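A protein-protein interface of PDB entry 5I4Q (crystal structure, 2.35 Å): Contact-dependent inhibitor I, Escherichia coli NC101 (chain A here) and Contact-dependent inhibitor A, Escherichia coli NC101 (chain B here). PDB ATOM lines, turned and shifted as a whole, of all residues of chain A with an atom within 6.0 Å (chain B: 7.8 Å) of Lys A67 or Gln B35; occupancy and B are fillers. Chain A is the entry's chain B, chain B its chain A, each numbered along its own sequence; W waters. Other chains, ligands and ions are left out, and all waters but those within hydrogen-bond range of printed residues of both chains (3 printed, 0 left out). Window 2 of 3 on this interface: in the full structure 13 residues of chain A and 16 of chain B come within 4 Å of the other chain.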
ATOM      1  N   GLN A  58     -10.865 -24.642  -3.258  1.00  0.00           N
ATOM      2  CA  GLN A  58      -9.562 -24.315  -2.785  1.00  0.00           C
ATOM      3  C   GLN A  58      -9.690 -23.282  -1.668  1.00  0.00           C
ATOM      4  O   GLN A  58      -9.006 -23.377  -0.683  1.00  0.00           O
ATOM      5  CB  GLN A  58      -8.665 -23.822  -3.929  1.00  0.00           C
ATOM      6  CG  GLN A  58      -7.235 -23.376  -3.551  1.00  0.00           C
ATOM      7  CD  GLN A  58      -7.136 -22.064  -2.804  1.00  0.00           C
ATOM      8  OE1 GLN A  58      -8.037 -21.232  -2.843  1.00  0.00           O
ATOM      9  NE2 GLN A  58      -6.035 -21.870  -2.095  1.00  0.00           N
ATOM     10  N   SER A  59     -10.576 -22.308  -1.838  1.00  0.00           N
ATOM     11  CA  SER A  59     -10.753 -21.215  -0.853  1.00  0.00           C
ATOM     12  C   SER A  59     -11.234 -21.732   0.444  1.00  0.00           C
ATOM     13  O   SER A  59     -10.777 -21.274   1.488  1.00  0.00           O
ATOM     14  CB  SER A  59     -11.679 -20.122  -1.345  1.00  0.00           C
ATOM     15  OG  SER A  59     -11.073 -19.513  -2.486  1.00  0.00           O
ATOM     16  N   GLU A  60     -12.088 -22.735   0.398  1.00  0.00           N
ATOM     17  CA  GLU A  60     -12.565 -23.308   1.608  1.00  0.00           C
ATOM     18  C   GLU A  60     -11.447 -24.108   2.268  1.00  0.00           C
ATOM     19  O   GLU A  60     -11.364 -24.158   3.498  1.00  0.00           O
ATOM     20  CB  GLU A  60     -13.772 -24.190   1.319  1.00  0.00           C
ATOM     21  CG  GLU A  60     -14.976 -23.405   0.853  1.00  0.00           C
ATOM     22  CD  GLU A  60     -16.062 -24.252   0.139  1.00  0.00           C
ATOM     23  OE1 GLU A  60     -15.935 -25.482   0.020  1.00  0.00           O
ATOM     24  OE2 GLU A  60     -17.079 -23.663  -0.285  1.00  0.00           O
ATOM     25  N   ALA A  62      -8.281 -23.519   1.982  1.00  0.00           N
ATOM     26  CA  ALA A  62      -7.382 -22.519   2.544  1.00  0.00           C
ATOM     27  C   ALA A  62      -7.898 -21.969   3.887  1.00  0.00           C
ATOM     28  O   ALA A  62      -7.110 -21.746   4.805  1.00  0.00           O
ATOM     29  CB  ALA A  62      -7.201 -21.414   1.526  1.00  0.00           C
ATOM     30  N   THR A  63      -9.218 -21.788   4.013  1.00  0.00           N
ATOM     31  CA  THR A  63      -9.807 -21.350   5.248  1.00  0.00           C
ATOM     32  C   THR A  63      -9.559 -22.412   6.313  1.00  0.00           C
ATOM     33  O   THR A  63      -9.254 -22.123   7.488  1.00  0.00           O
ATOM     34  CB  THR A  63     -11.309 -21.039   5.067  1.00  0.00           C
ATOM     35  OG1 THR A  63     -11.468 -20.037   4.064  1.00  0.00           O
ATOM     36  CG2 THR A  63     -11.923 -20.503   6.321  1.00  0.00           C
ATOM     37  N   MET A  64      -9.684 -23.665   5.928  1.00  0.00           N
ATOM     38  CA  MET A  64      -9.400 -24.718   6.872  1.00  0.00           C
ATOM     39  C   MET A  64      -7.979 -24.638   7.398  1.00  0.00           C
ATOM     40  O   MET A  64      -7.740 -24.842   8.575  1.00  0.00           O
ATOM     41  CB  MET A  64      -9.565 -26.019   6.128  1.00  0.00           C
ATOM     42  CG  MET A  64      -8.999 -27.173   6.939  1.00  0.00           C
ATOM     43  SD  MET A  64      -9.026 -28.796   5.794  1.00  0.00           S
ATOM     44  CE  MET A  64      -7.420 -28.361   4.703  1.00  0.00           C
ATOM     45  N   LEU A  65      -7.020 -24.415   6.507  1.00  0.00           N
ATOM     46  CA  LEU A  65      -5.600 -24.419   6.866  1.00  0.00           C
ATOM     47  C   LEU A  65      -5.253 -23.199   7.763  1.00  0.00           C
ATOM     48  O   LEU A  65      -4.587 -23.323   8.793  1.00  0.00           O
ATOM     49  CB  LEU A  65      -4.750 -24.411   5.578  1.00  0.00           C
ATOM     50  CG  LEU A  65      -3.228 -24.380   5.762  1.00  0.00           C
ATOM     51  CD1 LEU A  65      -2.808 -25.544   6.646  1.00  0.00           C
ATOM     52  CD2 LEU A  65      -2.503 -24.418   4.404  1.00  0.00           C
ATOM     53  N   TYR A  66      -5.732 -22.032   7.377  1.00  0.00           N
ATOM     54  CA  TYR A  66      -5.260 -20.792   8.001  1.00  0.00           C
ATOM     55  C   TYR A  66      -6.169 -20.348   9.093  1.00  0.00           C
ATOM     56  O   TYR A  66      -5.680 -19.948  10.096  1.00  0.00           O
ATOM     57  CB  TYR A  66      -5.096 -19.700   6.950  1.00  0.00           C
ATOM     58  CG  TYR A  66      -4.065 -20.048   5.926  1.00  0.00           C
ATOM     59  CD1 TYR A  66      -2.740 -20.208   6.279  1.00  0.00           C
ATOM     60  CD2 TYR A  66      -4.410 -20.229   4.619  1.00  0.00           C
ATOM     61  CE1 TYR A  66      -1.782 -20.553   5.329  1.00  0.00           C
ATOM     62  CE2 TYR A  66      -3.468 -20.586   3.663  1.00  0.00           C
ATOM     63  CZ  TYR A  66      -2.171 -20.755   4.016  1.00  0.00           C
ATOM     64  OH  TYR A  66      -1.266 -21.079   3.023  1.00  0.00           O
ATOM     65  N   LYS A  67      -7.488 -20.452   8.956  1.00  0.00           N
ATOM     66  CA  LYS A  67      -8.349 -20.011  10.052  1.00  0.00           C
ATOM     67  C   LYS A  67      -8.445 -21.036  11.171  1.00  0.00           C
ATOM     68  O   LYS A  67      -8.407 -20.679  12.329  1.00  0.00           O
ATOM     69  CB  LYS A  67      -9.725 -19.653   9.551  1.00  0.00           C
ATOM     70  CG  LYS A  67     -10.578 -18.875  10.518  1.00  0.00           C
ATOM     71  CD  LYS A  67     -11.839 -18.393   9.819  1.00  0.00           C
ATOM     72  CE  LYS A  67     -12.912 -17.994  10.806  1.00  0.00           C
ATOM     73  NZ  LYS A  67     -12.381 -16.999  11.783  1.00  0.00           N
ATOM     74  N   TYR A  68      -8.631 -22.307  10.833  1.00  0.00           N
ATOM     75  CA  TYR A  68      -8.892 -23.309  11.843  1.00  0.00           C
ATOM     76  C   TYR A  68      -7.657 -24.135  12.134  1.00  0.00           C
ATOM     77  O   TYR A  68      -7.683 -24.927  13.007  1.00  0.00           O
ATOM     78  CB  TYR A  68     -10.049 -24.214  11.400  1.00  0.00           C
ATOM     79  CG  TYR A  68     -11.285 -23.433  11.240  1.00  0.00           C
ATOM     80  CD1 TYR A  68     -11.984 -23.014  12.342  1.00  0.00           C
ATOM     81  CD2 TYR A  68     -11.737 -23.076   9.987  1.00  0.00           C
ATOM     82  CE1 TYR A  68     -13.073 -22.202  12.214  1.00  0.00           C
ATOM     83  CE2 TYR A  68     -12.855 -22.313   9.853  1.00  0.00           C
ATOM     84  CZ  TYR A  68     -13.496 -21.869  10.969  1.00  0.00           C
ATOM     85  OH  TYR A  68     -14.613 -21.117  10.846  1.00  0.00           O
ATOM     86  N   GLU A  69      -6.637 -23.995  11.327  1.00  0.00           N
ATOM     87  CA  GLU A  69      -5.349 -24.660  11.536  1.00  0.00           C
ATOM     88  C   GLU A  69      -5.403 -26.169  11.482  1.00  0.00           C
ATOM     89  O   GLU A  69      -4.734 -26.845  12.241  1.00  0.00           O
ATOM     90  CB  GLU A  69      -4.653 -24.114  12.795  1.00  0.00           C
ATOM     91  CG  GLU A  69      -4.246 -22.650  12.533  1.00  0.00           C
ATOM     92  CD  GLU A  69      -3.498 -22.034  13.704  1.00  0.00           C
ATOM     93  OE1 GLU A  69      -4.131 -21.784  14.731  1.00  0.00           O
ATOM     94  OE2 GLU A  69      -2.263 -21.830  13.593  1.00  0.00           O
ATOM     95  N   ASP A  84      -4.200 -21.371  -5.284  1.00  0.00           N
ATOM     96  CA  ASP A  84      -4.593 -20.192  -4.521  1.00  0.00           C
ATOM     97  C   ASP A  84      -4.871 -18.997  -5.405  1.00  0.00           C
ATOM     98  O   ASP A  84      -5.861 -18.323  -5.258  1.00  0.00           O
ATOM     99  CB  ASP A  84      -3.488 -19.802  -3.514  1.00  0.00           C
ATOM    100  CG  ASP A  84      -3.993 -18.850  -2.475  1.00  0.00           C
ATOM    101  OD1 ASP A  84      -4.854 -19.264  -1.672  1.00  0.00           O
ATOM    102  OD2 ASP A  84      -3.645 -17.675  -2.499  1.00  0.00           O
ATOM    103  N   TYR B  28     -10.497  -8.972  -2.994  1.00  0.00           N
ATOM    104  CA  TYR B  28      -9.336  -9.745  -2.569  1.00  0.00           C
ATOM    105  C   TYR B  28      -8.978  -9.371  -1.124  1.00  0.00           C
ATOM    106  O   TYR B  28      -8.776 -10.244  -0.278  1.00  0.00           O
ATOM    107  CB  TYR B  28      -8.149  -9.601  -3.522  1.00  0.00           C
ATOM    108  CG  TYR B  28      -7.042 -10.566  -3.242  1.00  0.00           C
ATOM    109  CD1 TYR B  28      -7.298 -11.939  -3.113  1.00  0.00           C
ATOM    110  CD2 TYR B  28      -5.745 -10.140  -3.147  1.00  0.00           C
ATOM    111  CE1 TYR B  28      -6.282 -12.852  -2.840  1.00  0.00           C
ATOM    112  CE2 TYR B  28      -4.712 -11.027  -2.858  1.00  0.00           C
ATOM    113  CZ  TYR B  28      -4.968 -12.379  -2.714  1.00  0.00           C
ATOM    114  OH  TYR B  28      -3.924 -13.235  -2.432  1.00  0.00           O
ATOM    115  N   TYR B  29      -9.037  -8.075  -0.828  1.00  0.00           N
ATOM    116  CA  TYR B  29      -8.780  -7.594   0.515  1.00  0.00           C
ATOM    117  C   TYR B  29      -9.679  -8.280   1.540  1.00  0.00           C
ATOM    118  O   TYR B  29      -9.208  -8.781   2.563  1.00  0.00           O
ATOM    119  CB  TYR B  29      -8.966  -6.078   0.582  1.00  0.00           C
ATOM    120  CG  TYR B  29      -8.645  -5.487   1.936  1.00  0.00           C
ATOM    121  CD1 TYR B  29      -7.351  -5.273   2.326  1.00  0.00           C
ATOM    122  CD2 TYR B  29      -9.654  -5.128   2.812  1.00  0.00           C
ATOM    123  CE1 TYR B  29      -7.048  -4.716   3.561  1.00  0.00           C
ATOM    124  CE2 TYR B  29      -9.360  -4.547   4.060  1.00  0.00           C
ATOM    125  CZ  TYR B  29      -8.062  -4.325   4.425  1.00  0.00           C
ATOM    126  OH  TYR B  29      -7.766  -3.757   5.679  1.00  0.00           O
ATOM    127  N   GLU B  30     -10.953  -8.337   1.245  1.00  0.00           N
ATOM    128  CA  GLU B  30     -11.903  -8.889   2.211  1.00  0.00           C
ATOM    129  C   GLU B  30     -11.736 -10.387   2.352  1.00  0.00           C
ATOM    130  O   GLU B  30     -11.928 -10.954   3.453  1.00  0.00           O
ATOM    131  CB  GLU B  30     -13.333  -8.485   1.800  1.00  0.00           C
ATOM    132  CG  GLU B  30     -13.459  -6.974   1.927  1.00  0.00           C
ATOM    133  CD  GLU B  30     -14.757  -6.368   1.378  1.00  0.00           C
ATOM    134  OE1 GLU B  30     -15.580  -7.115   0.840  1.00  0.00           O
ATOM    135  OE2 GLU B  30     -14.932  -5.121   1.488  1.00  0.00           O
ATOM    136  N   LYS B  31     -11.356 -11.021   1.242  1.00  0.00           N
ATOM    137  CA  LYS B  31     -11.194 -12.464   1.204  1.00  0.00           C
ATOM    138  C   LYS B  31     -10.061 -12.887   2.131  1.00  0.00           C
ATOM    139  O   LYS B  31     -10.171 -13.840   2.829  1.00  0.00           O
ATOM    140  CB  LYS B  31     -10.864 -12.905  -0.209  1.00  0.00           C
ATOM    141  CG  LYS B  31     -10.886 -14.416  -0.416  1.00  0.00           C
ATOM    142  CD  LYS B  31     -10.258 -14.789  -1.771  1.00  0.00           C
ATOM    143  CE  LYS B  31     -10.123 -16.297  -1.876  1.00  0.00           C
ATOM    144  NZ  LYS B  31      -9.895 -16.834  -3.241  1.00  0.00           N
ATOM    145  N   LEU B  32      -8.961 -12.148   2.106  1.00  0.00           N
ATOM    146  CA  LEU B  32      -7.815 -12.458   2.928  1.00  0.00           C
ATOM    147  C   LEU B  32      -8.156 -12.401   4.397  1.00  0.00           C
ATOM    148  O   LEU B  32      -7.970 -13.360   5.096  1.00  0.00           O
ATOM    149  CB  LEU B  32      -6.684 -11.524   2.552  1.00  0.00           C
ATOM    150  CG  LEU B  32      -5.972 -11.831   1.225  1.00  0.00           C
ATOM    151  CD1 LEU B  32      -4.985 -10.731   0.936  1.00  0.00           C
ATOM    152  CD2 LEU B  32      -5.169 -13.096   1.231  1.00  0.00           C
ATOM    153  N   TRP B  33      -8.785 -11.342   4.866  1.00  0.00           N
ATOM    154  CA  TRP B  33      -9.231 -11.347   6.291  1.00  0.00           C
ATOM    155  C   TRP B  33     -10.201 -12.487   6.615  1.00  0.00           C
ATOM    156  O   TRP B  33     -10.120 -13.126   7.628  1.00  0.00           O
ATOM    157  CB  TRP B  33      -9.944 -10.044   6.606  1.00  0.00           C
ATOM    158  CG  TRP B  33      -9.003  -8.864   6.743  1.00  0.00           C
ATOM    159  CD1 TRP B  33      -8.567  -8.025   5.750  1.00  0.00           C
ATOM    160  CD2 TRP B  33      -8.469  -8.359   7.969  1.00  0.00           C
ATOM    161  NE1 TRP B  33      -7.767  -7.022   6.312  1.00  0.00           N
ATOM    162  CE2 TRP B  33      -7.713  -7.216   7.670  1.00  0.00           C
ATOM    163  CE3 TRP B  33      -8.564  -8.767   9.289  1.00  0.00           C
ATOM    164  CZ2 TRP B  33      -7.048  -6.499   8.640  1.00  0.00           C
ATOM    165  CZ3 TRP B  33      -7.902  -8.028  10.275  1.00  0.00           C
ATOM    166  CH2 TRP B  33      -7.149  -6.923   9.938  1.00  0.00           C
ATOM    167  N   GLU B  34     -11.114 -12.751   5.704  1.00  0.00           N
ATOM    168  CA  GLU B  34     -12.110 -13.756   5.896  1.00  0.00           C
ATOM    169  C   GLU B  34     -11.506 -15.131   5.941  1.00  0.00           C
ATOM    170  O   GLU B  34     -11.965 -15.934   6.659  1.00  0.00           O
ATOM    171  CB  GLU B  34     -13.156 -13.654   4.794  1.00  0.00           C
ATOM    172  CG  GLU B  34     -14.464 -14.318   5.135  1.00  0.00           C
ATOM    173  CD  GLU B  34     -15.472 -14.180   3.986  1.00  0.00           C
ATOM    174  OE1 GLU B  34     -15.109 -13.576   2.938  1.00  0.00           O
ATOM    175  OE2 GLU B  34     -16.617 -14.692   4.120  1.00  0.00           O
ATOM    176  N   GLN B  35     -10.456 -15.394   5.202  1.00  0.00           N
ATOM    177  CA  GLN B  35      -9.886 -16.746   5.161  1.00  0.00           C
ATOM    178  C   GLN B  35      -8.849 -17.019   6.246  1.00  0.00           C
ATOM    179  O   GLN B  35      -8.233 -18.079   6.272  1.00  0.00           O
ATOM    180  CB  GLN B  35      -9.132 -16.960   3.903  1.00  0.00           C
ATOM    181  CG  GLN B  35      -9.945 -17.209   2.701  1.00  0.00           C
ATOM    182  CD  GLN B  35      -9.028 -17.757   1.599  1.00  0.00           C
ATOM    183  OE1 GLN B  35      -7.792 -17.706   1.727  1.00  0.00           O
ATOM    184  NE2 GLN B  35      -9.628 -18.308   0.539  1.00  0.00           N
ATOM    185  N   GLY B  36      -8.624 -16.066   7.123  1.00  0.00           N
ATOM    186  CA  GLY B  36      -7.687 -16.286   8.178  1.00  0.00           C
ATOM    187  C   GLY B  36      -6.284 -15.840   7.825  1.00  0.00           C
ATOM    188  O   GLY B  36      -5.325 -16.312   8.455  1.00  0.00           O
ATOM    189  N   ARG B  37      -6.169 -14.925   6.849  1.00  0.00           N
ATOM    190  CA  ARG B  37      -4.894 -14.296   6.505  1.00  0.00           C
ATOM    191  C   ARG B  37      -4.960 -12.777   6.683  1.00  0.00           C
ATOM    192  O   ARG B  37      -4.979 -12.022   5.708  1.00  0.00           O
ATOM    193  CB  ARG B  37      -4.477 -14.669   5.102  1.00  0.00           C
ATOM    194  CG  ARG B  37      -4.012 -16.124   5.036  1.00  0.00           C
ATOM    195  CD  ARG B  37      -4.506 -16.820   3.796  1.00  0.00           C
ATOM    196  NE  ARG B  37      -3.655 -16.540   2.650  1.00  0.00           N
ATOM    197  CZ  ARG B  37      -3.849 -17.068   1.452  1.00  0.00           C
ATOM    198  NH1 ARG B  37      -4.869 -17.899   1.223  1.00  0.00           N
ATOM    199  NH2 ARG B  37      -3.031 -16.751   0.481  1.00  0.00           N
ATOM    200  N   PRO B  38      -5.069 -12.328   7.940  1.00  0.00           N
ATOM    201  CA  PRO B  38      -5.322 -10.932   8.203  1.00  0.00           C
ATOM    202  C   PRO B  38      -4.110 -10.046   7.947  1.00  0.00           C
ATOM    203  O   PRO B  38      -2.983 -10.524   7.727  1.00  0.00           O
ATOM    204  CB  PRO B  38      -5.683 -10.914   9.687  1.00  0.00           C
ATOM    205  CG  PRO B  38      -4.928 -12.101  10.241  1.00  0.00           C
ATOM    206  CD  PRO B  38      -5.080 -13.133   9.187  1.00  0.00           C
ATOM    207  N   ILE B  86      -1.029 -12.693  -2.842  1.00  0.00           N
ATOM    208  CA  ILE B  86      -0.048 -12.919  -1.822  1.00  0.00           C
ATOM    209  C   ILE B  86      -0.467 -14.185  -1.019  1.00  0.00           C
ATOM    210  O   ILE B  86      -1.622 -14.350  -0.701  1.00  0.00           O
ATOM    211  CB  ILE B  86       0.079 -11.685  -0.916  1.00  0.00           C
ATOM    212  CG1 ILE B  86       1.170 -11.870   0.126  1.00  0.00           C
ATOM    213  CG2 ILE B  86      -1.233 -11.358  -0.267  1.00  0.00           C
ATOM    214  CD1 ILE B  86       1.774 -10.554   0.611  1.00  0.00           C
HETATM  215  O   HOH W   1      -8.586 -19.288  -4.978  1.00  0.00           O
HETATM  216  O   HOH W   2      -4.740 -15.517  -1.766  1.00  0.00           O
HETATM  217  O   HOH W   3      -7.784 -18.883  -1.706  1.00  0.00           O
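Ala A62 touches Gln B35. Gln B35 touches Thr A63. CB of Tyr A66 touches O of Gln B35 (3.6 Å). O of Gly B36 touches CB of Tyr A66, at 3.7 Å. Arg B37 touches Tyr A66. Gln B35 touches Lys A67 (O to N, 3.7 Å).
The side-chain amino group of Lys B31 sits at hydrogen-bond distance from the side-chain hydroxyl of Ser A59 (3.0 Å). NE2 of Gln B35 is in hydrogen-bond range of O of Ser A59 (3.3 Å). The side-chain carboxylate (OD2) of Asp A84 is in salt-bridge range of the guanidinium group (NH2) of Arg B37 (3.2 Å).
Water W2 lies within hydrogen-bond range of the side-chain hydroxyl (OH) of Tyr B28 (2.5 Å), the side-chain carboxylate (OD2) of Asp A84 (2.5 Å), the guanidinium group (NH2) of Arg B37 (3.1 Å) and the backbone carbonyl oxygen (O) of Ile B86 (3.5 Å). Water W3 lies within hydrogen-bond range of OE1 of Gln A58 (2.6 Å), OD1 of Asp A84 (3.0 Å), NE2 of Gln B35 (3.0 Å), NZ of Lys B31 (3.3 Å) and OG of Ser A59 (3.4 Å). Water W1 lies within hydrogen-bond range of O of Asp A84 (2.9 Å), OE1 of Gln A58 (2.9 Å) and NZ of Lys B31 (3.3 Å).
Of the 12 printed residues of chain B, 4 touch a printed residue of chain A. Printed residues of chain B that touch a printed residue of chain A: Lys B31, Gln B35, Gly B36 and Arg B37. Of the 12 printed residues of chain A, 6 touch a printed residue of chain B. Hydrophobic or aromatic side chains of chain A within 4 Å of the printed part of chain B: Ala A62 and Tyr A66. Among the printed residues, 9 pairs touch across the chains.
O of Leu B32 is in hydrogen-bond range of N of Arg B37. The side-chain amide oxygen (OE1) of Gln B35 lies within hydrogen-bond range of the guanidinium group (NH1) of Arg B37, 3.0 Å away. O of Ile B86 lies within hydrogen-bond range of NH2 of Arg B37, at 3.0 Å. The side-chain carboxylate of Asp A84 lies within hydrogen-bond range of the side-chain amide nitrogen of Gln A58, at 2.9 Å. OG1 of Thr A63 sits at hydrogen-bond distance from O of Ser A59. The backbone NH of Tyr A68 is in hydrogen-bond range of the backbone carbonyl oxygen of Thr A63 (3.4 Å).
Of the printed residues of chain B, Ala A62 touches Gln B35. Of the printed residues of chain B, Tyr A66 touches Gln B35, Gly B36 and Arg B37. Printed residues of chain B within 4 Å of Asp A84: Arg B37. Gln B35 touches five residues of chain A. Of the printed residues of chain A, Arg B37 touches Tyr A66 and Asp A84. Ile B86 touches none of the printed residues of chain A.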
